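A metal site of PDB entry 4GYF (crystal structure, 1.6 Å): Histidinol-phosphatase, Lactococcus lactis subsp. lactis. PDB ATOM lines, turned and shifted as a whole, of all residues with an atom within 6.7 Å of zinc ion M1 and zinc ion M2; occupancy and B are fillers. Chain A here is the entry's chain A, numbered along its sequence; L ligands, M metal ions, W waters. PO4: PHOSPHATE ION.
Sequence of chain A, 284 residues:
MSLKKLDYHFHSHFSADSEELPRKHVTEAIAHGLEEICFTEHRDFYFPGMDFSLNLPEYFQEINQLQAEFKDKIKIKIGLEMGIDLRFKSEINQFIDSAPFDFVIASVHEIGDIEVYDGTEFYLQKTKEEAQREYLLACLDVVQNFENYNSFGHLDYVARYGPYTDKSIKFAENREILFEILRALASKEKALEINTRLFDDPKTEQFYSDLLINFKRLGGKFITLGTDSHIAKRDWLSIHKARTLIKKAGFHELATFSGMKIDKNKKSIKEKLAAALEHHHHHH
OG of Ser 107 lies close to OE2 of Glu 81 (2.9 Å).
The backbone NH of His 154 sits at hydrogen-bond distance from the side-chain carboxylate of Glu 193 (2.9 Å).
A ring nitrogen (ND1) of His 9 sits at hydrogen-bond distance from the side-chain carboxylate of Glu 193 (2.7 Å).
A ring nitrogen (ND1) of His 11 lies close to the backbone carbonyl oxygen (O) of Thr 40.
The backbone NH of His 11 lies within hydrogen-bond range of the backbone carbonyl oxygen of Ser 229.
The backbone carbonyl oxygen (O) of Asp 228 sits at hydrogen-bond distance from a ring nitrogen (ND1) of His 230, 2.9 Å away.
NH2 of Arg 160 lies within salt-bridge range of OD2 of Asp 228.
The guanidinium group (NH2) of Arg 197 lies within salt-bridge range of the side-chain carboxylate (OD2) of Asp 228, 3.7 Å away.
Residues that only touch zinc ion M1: Ser 107 (3.9 Å).
Within 4 Å of zinc ion M1: Glu 81, Ser 107, His 109 and His 154.
CE1 of His 42 touches zinc ion M2 (3.8 Å).
The nearest printed residue that does not touch zinc ion M2 is His 230 (4.2 Å).
Zinc ion M1 is bound by OE2 of Glu 81 (2.0 Å), NE2 of His 109 (2.1 Å), NE2 of His 154 (2.1 Å), water W1 (2.1 Å) and O3 of the ligand (2.2 Å).
Zinc ion M2 is bound by O1 of the ligand (1.9 Å).
Water W1 is bound to zinc ion M2, at 2.1 Å.
NE2 of His 9 is bound to zinc ion M2.
NE2 of His 11 is bound to zinc ion M2, 2.2 Å away.
Zinc ion M2 is bound by OE1 of Glu 81.
OD1 of Asp 228 is bound to zinc ion M2.
Zinc ion M2 has six donor atoms within binding distance.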
ATOM      1  N   HIS A   9     -21.087 -14.622  14.473  1.00  0.00           N
ATOM      2  CA  HIS A   9     -20.618 -15.538  13.422  1.00  0.00           C
ATOM      3  C   HIS A   9     -21.437 -16.806  13.425  1.00  0.00           C
ATOM      4  O   HIS A   9     -21.253 -17.655  14.300  1.00  0.00           O
ATOM      5  CB  HIS A   9     -19.130 -15.885  13.615  1.00  0.00           C
ATOM      6  CG  HIS A   9     -18.527 -16.587  12.438  1.00  0.00           C
ATOM      7  ND1 HIS A   9     -17.178 -16.512  12.148  1.00  0.00           N
ATOM      8  CD2 HIS A   9     -19.068 -17.370  11.474  1.00  0.00           C
ATOM      9  CE1 HIS A   9     -16.917 -17.213  11.061  1.00  0.00           C
ATOM     10  NE2 HIS A   9     -18.043 -17.765  10.640  1.00  0.00           N
ATOM     11  N   PHE A  10     -22.310 -16.961  12.435  1.00  0.00           N
ATOM     12  CA  PHE A  10     -23.073 -18.208  12.329  1.00  0.00           C
ATOM     13  C   PHE A  10     -23.748 -18.295  10.970  1.00  0.00           C
ATOM     14  O   PHE A  10     -23.829 -17.302  10.240  1.00  0.00           O
ATOM     15  CB  PHE A  10     -24.083 -18.363  13.474  1.00  0.00           C
ATOM     16  CG  PHE A  10     -25.107 -17.270  13.546  1.00  0.00           C
ATOM     17  CD1 PHE A  10     -26.339 -17.403  12.912  1.00  0.00           C
ATOM     18  CD2 PHE A  10     -24.859 -16.119  14.295  1.00  0.00           C
ATOM     19  CE1 PHE A  10     -27.288 -16.394  12.984  1.00  0.00           C
ATOM     20  CE2 PHE A  10     -25.808 -15.118  14.388  1.00  0.00           C
ATOM     21  CZ  PHE A  10     -27.031 -15.251  13.725  1.00  0.00           C
ATOM     22  N   HIS A  11     -24.211 -19.492  10.628  1.00  0.00           N
ATOM     23  CA  HIS A  11     -24.627 -19.789   9.258  1.00  0.00           C
ATOM     24  C   HIS A  11     -25.982 -20.479   9.238  1.00  0.00           C
ATOM     25  O   HIS A  11     -26.283 -21.279  10.121  1.00  0.00           O
ATOM     26  CB  HIS A  11     -23.599 -20.714   8.574  1.00  0.00           C
ATOM     27  CG  HIS A  11     -22.231 -20.129   8.493  1.00  0.00           C
ATOM     28  ND1 HIS A  11     -21.767 -19.503   7.353  1.00  0.00           N
ATOM     29  CD2 HIS A  11     -21.239 -20.065   9.401  1.00  0.00           C
ATOM     30  CE1 HIS A  11     -20.534 -19.066   7.574  1.00  0.00           C
ATOM     31  NE2 HIS A  11     -20.189 -19.398   8.803  1.00  0.00           N
ATOM     32  N   ASP A  17     -22.935 -24.755   3.054  1.00  0.00           N
ATOM     33  CA  ASP A  17     -22.641 -25.875   3.958  1.00  0.00           C
ATOM     34  C   ASP A  17     -23.498 -25.874   5.232  1.00  0.00           C
ATOM     35  O   ASP A  17     -23.121 -26.478   6.249  1.00  0.00           O
ATOM     36  CB  ASP A  17     -21.153 -25.865   4.331  1.00  0.00           C
ATOM     37  CG  ASP A  17     -20.748 -24.636   5.146  1.00  0.00           C
ATOM     38  OD1 ASP A  17     -21.565 -23.708   5.245  1.00  0.00           O
ATOM     39  OD2 ASP A  17     -19.613 -24.592   5.679  1.00  0.00           O
ATOM     40  N   THR A  40     -23.890 -14.396   9.285  1.00  0.00           N
ATOM     41  CA  THR A  40     -22.677 -14.189   8.500  1.00  0.00           C
ATOM     42  C   THR A  40     -22.525 -15.310   7.471  1.00  0.00           C
ATOM     43  O   THR A  40     -21.687 -16.212   7.639  1.00  0.00           O
ATOM     44  CB  THR A  40     -21.400 -14.095   9.376  1.00  0.00           C
ATOM     45  OG1 THR A  40     -21.244 -15.293  10.146  1.00  0.00           O
ATOM     46  CG2 THR A  40     -21.452 -12.894  10.340  1.00  0.00           C
ATOM     47  N   HIS A  42     -21.783 -17.570   4.071  1.00  0.00           N
ATOM     48  CA  HIS A  42     -20.581 -17.738   3.248  1.00  0.00           C
ATOM     49  C   HIS A  42     -20.726 -17.159   1.850  1.00  0.00           C
ATOM     50  O   HIS A  42     -21.722 -17.414   1.157  1.00  0.00           O
ATOM     51  CB  HIS A  42     -20.290 -19.220   3.025  1.00  0.00           C
ATOM     52  CG  HIS A  42     -19.716 -19.956   4.190  1.00  0.00           C
ATOM     53  ND1 HIS A  42     -18.504 -19.629   4.768  1.00  0.00           N
ATOM     54  CD2 HIS A  42     -20.142 -21.073   4.826  1.00  0.00           C
ATOM     55  CE1 HIS A  42     -18.230 -20.501   5.732  1.00  0.00           C
ATOM     56  NE2 HIS A  42     -19.215 -21.382   5.785  1.00  0.00           N
ATOM     57  N   GLU A  81     -19.616 -13.734   5.729  1.00  0.00           N
ATOM     58  CA  GLU A  81     -18.272 -14.275   5.879  1.00  0.00           C
ATOM     59  C   GLU A  81     -17.680 -14.438   4.507  1.00  0.00           C
ATOM     60  O   GLU A  81     -18.065 -15.323   3.743  1.00  0.00           O
ATOM     61  CB  GLU A  81     -18.240 -15.626   6.602  1.00  0.00           C
ATOM     62  CG  GLU A  81     -16.774 -16.086   6.839  1.00  0.00           C
ATOM     63  CD  GLU A  81     -16.629 -17.497   7.407  1.00  0.00           C
ATOM     64  OE1 GLU A  81     -17.650 -18.183   7.638  1.00  0.00           O
ATOM     65  OE2 GLU A  81     -15.477 -17.933   7.617  1.00  0.00           O
ATOM     66  N   ILE A 105     -16.793 -10.439   7.776  1.00  0.00           N
ATOM     67  CA  ILE A 105     -15.636 -11.170   8.297  1.00  0.00           C
ATOM     68  C   ILE A 105     -14.766 -11.550   7.106  1.00  0.00           C
ATOM     69  O   ILE A 105     -15.283 -12.057   6.111  1.00  0.00           O
ATOM     70  CB  ILE A 105     -16.080 -12.478   8.968  1.00  0.00           C
ATOM     71  CG1 ILE A 105     -16.978 -12.196  10.181  1.00  0.00           C
ATOM     72  CG2 ILE A 105     -14.870 -13.322   9.377  1.00  0.00           C
ATOM     73  CD1 ILE A 105     -17.636 -13.456  10.739  1.00  0.00           C
ATOM     74  N   SER A 107     -11.995 -14.166   5.905  1.00  0.00           N
ATOM     75  CA  SER A 107     -11.485 -15.470   6.308  1.00  0.00           C
ATOM     76  C   SER A 107     -10.611 -16.074   5.220  1.00  0.00           C
ATOM     77  O   SER A 107     -10.779 -15.769   4.031  1.00  0.00           O
ATOM     78  CB  SER A 107     -12.659 -16.408   6.566  1.00  0.00           C
ATOM     79  OG  SER A 107     -13.345 -16.026   7.736  1.00  0.00           O
ATOM     80  N   VAL A 108      -9.699 -16.953   5.627  1.00  0.00           N
ATOM     81  CA  VAL A 108      -8.948 -17.736   4.658  1.00  0.00           C
ATOM     82  C   VAL A 108      -9.411 -19.188   4.761  1.00  0.00           C
ATOM     83  O   VAL A 108      -9.307 -19.810   5.824  1.00  0.00           O
ATOM     84  CB  VAL A 108      -7.434 -17.646   4.884  1.00  0.00           C
ATOM     85  CG1 VAL A 108      -6.683 -18.607   3.944  1.00  0.00           C
ATOM     86  CG2 VAL A 108      -6.949 -16.233   4.642  1.00  0.00           C
ATOM     87  N   HIS A 109      -9.929 -19.698   3.640  1.00  0.00           N
ATOM     88  CA  HIS A 109     -10.452 -21.069   3.560  1.00  0.00           C
ATOM     89  C   HIS A 109      -9.715 -21.928   2.544  1.00  0.00           C
ATOM     90  O   HIS A 109      -9.792 -23.165   2.593  1.00  0.00           O
ATOM     91  CB  HIS A 109     -11.936 -21.037   3.188  1.00  0.00           C
ATOM     92  CG  HIS A 109     -12.822 -20.438   4.241  1.00  0.00           C
ATOM     93  ND1 HIS A 109     -13.876 -19.615   3.928  1.00  0.00           N
ATOM     94  CD2 HIS A 109     -12.812 -20.559   5.595  1.00  0.00           C
ATOM     95  CE1 HIS A 109     -14.493 -19.251   5.055  1.00  0.00           C
ATOM     96  NE2 HIS A 109     -13.868 -19.810   6.070  1.00  0.00           N
ATOM     97  N   GLY A 153     -11.463 -13.419  10.589  1.00  0.00           N
ATOM     98  CA  GLY A 153     -12.029 -14.657  11.090  1.00  0.00           C
ATOM     99  C   GLY A 153     -11.057 -15.753  11.482  1.00  0.00           C
ATOM    100  O   GLY A 153      -9.960 -15.885  10.910  1.00  0.00           O
ATOM    101  N   HIS A 154     -11.480 -16.554  12.455  1.00  0.00           N
ATOM    102  CA  HIS A 154     -10.771 -17.761  12.915  1.00  0.00           C
ATOM    103  C   HIS A 154      -9.293 -17.948  12.566  1.00  0.00           C
ATOM    104  O   HIS A 154      -8.962 -18.732  11.675  1.00  0.00           O
ATOM    105  CB  HIS A 154     -11.576 -19.025  12.537  1.00  0.00           C
ATOM    106  CG  HIS A 154     -12.026 -19.076  11.097  1.00  0.00           C
ATOM    107  ND1 HIS A 154     -11.193 -18.840  10.027  1.00  0.00           N
ATOM    108  CD2 HIS A 154     -13.230 -19.399  10.573  1.00  0.00           C
ATOM    109  CE1 HIS A 154     -11.872 -18.998   8.896  1.00  0.00           C
ATOM    110  NE2 HIS A 154     -13.108 -19.344   9.204  1.00  0.00           N
ATOM    111  N   TYR A 157      -8.152 -21.534  12.335  1.00  0.00           N
ATOM    112  CA  TYR A 157      -8.855 -22.397  11.376  1.00  0.00           C
ATOM    113  C   TYR A 157      -8.038 -23.636  11.004  1.00  0.00           C
ATOM    114  O   TYR A 157      -8.569 -24.751  10.924  1.00  0.00           O
ATOM    115  CB  TYR A 157      -9.190 -21.589  10.114  1.00  0.00           C
ATOM    116  CG  TYR A 157     -10.050 -22.283   9.080  1.00  0.00           C
ATOM    117  CD1 TYR A 157     -11.433 -22.294   9.195  1.00  0.00           C
ATOM    118  CD2 TYR A 157      -9.475 -22.864   7.959  1.00  0.00           C
ATOM    119  CE1 TYR A 157     -12.227 -22.894   8.213  1.00  0.00           C
ATOM    120  CE2 TYR A 157     -10.252 -23.474   6.993  1.00  0.00           C
ATOM    121  CZ  TYR A 157     -11.627 -23.486   7.130  1.00  0.00           C
ATOM    122  OH  TYR A 157     -12.393 -24.089   6.156  1.00  0.00           O
ATOM    123  N   ARG A 160      -8.298 -26.857  13.028  1.00  0.00           N
ATOM    124  CA  ARG A 160      -9.521 -27.664  13.055  1.00  0.00           C
ATOM    125  C   ARG A 160      -9.327 -28.982  12.338  1.00  0.00           C
ATOM    126  O   ARG A 160     -10.036 -29.982  12.603  1.00  0.00           O
ATOM    127  CB  ARG A 160     -10.670 -26.908  12.381  1.00  0.00           C
ATOM    128  CG  ARG A 160     -11.035 -25.568  13.008  1.00  0.00           C
ATOM    129  CD  ARG A 160     -12.031 -24.886  12.086  1.00  0.00           C
ATOM    130  NE  ARG A 160     -12.657 -23.726  12.699  1.00  0.00           N
ATOM    131  CZ  ARG A 160     -13.705 -23.102  12.178  1.00  0.00           C
ATOM    132  NH1 ARG A 160     -14.245 -23.540  11.051  1.00  0.00           N
ATOM    133  NH2 ARG A 160     -14.225 -22.049  12.799  1.00  0.00           N
ATOM    134  N   GLU A 193     -11.506 -11.624  15.494  1.00  0.00           N
ATOM    135  CA  GLU A 193     -12.587 -12.517  15.904  1.00  0.00           C
ATOM    136  C   GLU A 193     -12.135 -13.546  16.927  1.00  0.00           C
ATOM    137  O   GLU A 193     -11.123 -14.215  16.731  1.00  0.00           O
ATOM    138  CB  GLU A 193     -13.166 -13.254  14.701  1.00  0.00           C
ATOM    139  CG  GLU A 193     -14.150 -14.331  15.106  1.00  0.00           C
ATOM    140  CD  GLU A 193     -14.748 -15.053  13.919  1.00  0.00           C
ATOM    141  OE1 GLU A 193     -14.130 -16.033  13.440  1.00  0.00           O
ATOM    142  OE2 GLU A 193     -15.844 -14.634  13.485  1.00  0.00           O
ATOM    143  N   ASN A 195     -13.341 -16.929  17.900  1.00  0.00           N
ATOM    144  CA  ASN A 195     -14.215 -17.941  17.317  1.00  0.00           C
ATOM    145  C   ASN A 195     -14.244 -19.137  18.243  1.00  0.00           C
ATOM    146  O   ASN A 195     -13.197 -19.698  18.578  1.00  0.00           O
ATOM    147  CB  ASN A 195     -13.651 -18.350  15.945  1.00  0.00           C
ATOM    148  CG  ASN A 195     -14.587 -19.259  15.169  1.00  0.00           C
ATOM    149  OD1 ASN A 195     -14.962 -20.346  15.633  1.00  0.00           O
ATOM    150  ND2 ASN A 195     -14.961 -18.826  13.964  1.00  0.00           N
ATOM    151  N   ARG A 197     -15.499 -22.210  17.977  1.00  0.00           N
ATOM    152  CA  ARG A 197     -15.646 -23.565  17.411  1.00  0.00           C
ATOM    153  C   ARG A 197     -14.883 -24.643  18.180  1.00  0.00           C
ATOM    154  O   ARG A 197     -15.438 -25.699  18.510  1.00  0.00           O
ATOM    155  CB  ARG A 197     -15.235 -23.584  15.937  1.00  0.00           C
ATOM    156  CG  ARG A 197     -15.192 -24.993  15.311  1.00  0.00           C
ATOM    157  CD  ARG A 197     -16.581 -25.567  15.054  1.00  0.00           C
ATOM    158  NE  ARG A 197     -17.293 -24.755  14.079  1.00  0.00           N
ATOM    159  CZ  ARG A 197     -17.100 -24.827  12.760  1.00  0.00           C
ATOM    160  NH1 ARG A 197     -16.220 -25.698  12.274  1.00  0.00           N
ATOM    161  NH2 ARG A 197     -17.766 -24.038  11.933  1.00  0.00           N
ATOM    162  N   ASP A 228     -19.589 -19.630  15.150  1.00  0.00           N
ATOM    163  CA  ASP A 228     -19.440 -20.311  13.865  1.00  0.00           C
ATOM    164  C   ASP A 228     -20.374 -21.524  13.773  1.00  0.00           C
ATOM    165  O   ASP A 228     -20.095 -22.472  13.042  1.00  0.00           O
ATOM    166  CB  ASP A 228     -17.993 -20.762  13.629  1.00  0.00           C
ATOM    167  CG  ASP A 228     -17.562 -20.613  12.183  1.00  0.00           C
ATOM    168  OD1 ASP A 228     -18.432 -20.551  11.269  1.00  0.00           O
ATOM    169  OD2 ASP A 228     -16.335 -20.573  11.952  1.00  0.00           O
ATOM    170  N   SER A 229     -21.490 -21.467  14.495  1.00  0.00           N
ATOM    171  CA  SER A 229     -22.421 -22.598  14.466  1.00  0.00           C
ATOM    172  C   SER A 229     -23.175 -22.652  13.137  1.00  0.00           C
ATOM    173  O   SER A 229     -23.654 -21.630  12.647  1.00  0.00           O
ATOM    174  CB  SER A 229     -23.416 -22.513  15.629  1.00  0.00           C
ATOM    175  OG  SER A 229     -24.096 -23.752  15.775  1.00  0.00           O
ATOM    176  N   HIS A 230     -23.268 -23.847  12.558  1.00  0.00           N
ATOM    177  CA  HIS A 230     -24.006 -24.039  11.315  1.00  0.00           C
ATOM    178  C   HIS A 230     -25.382 -24.645  11.623  1.00  0.00           C
ATOM    179  O   HIS A 230     -26.178 -24.915  10.717  1.00  0.00           O
ATOM    180  CB  HIS A 230     -23.211 -24.918  10.347  1.00  0.00           C
ATOM    181  CG  HIS A 230     -22.007 -24.241   9.752  1.00  0.00           C
ATOM    182  ND1 HIS A 230     -21.075 -23.587  10.524  1.00  0.00           N
ATOM    183  CD2 HIS A 230     -21.596 -24.110   8.477  1.00  0.00           C
ATOM    184  CE1 HIS A 230     -20.134 -23.077   9.748  1.00  0.00           C
ATOM    185  NE2 HIS A 230     -20.414 -23.394   8.490  1.00  0.00           N
HETATM  186  P   PO4 L   1     -16.795 -22.290   8.422  1.00  0.00           P
HETATM  187  O1  PO4 L   1     -17.823 -21.216   8.659  1.00  0.00           O
HETATM  188  O2  PO4 L   1     -16.365 -22.949   9.703  1.00  0.00           O
HETATM  189  O3  PO4 L   1     -15.596 -21.694   7.720  1.00  0.00           O
HETATM  190  O4  PO4 L   1     -17.430 -23.344   7.533  1.00  0.00           O
HETATM  191 ZN    ZN M   1     -14.741 -19.713   7.944  1.00  0.00          ZN
HETATM  192 ZN    ZN M   2     -18.100 -19.473   9.347  1.00  0.00          ZN
HETATM  193 ZN    ZN M   3     -19.242 -23.073   6.851  1.00  0.00          ZN
HETATM  194  O   HOH W   1     -15.998 -19.739   9.633  1.00  0.00           O
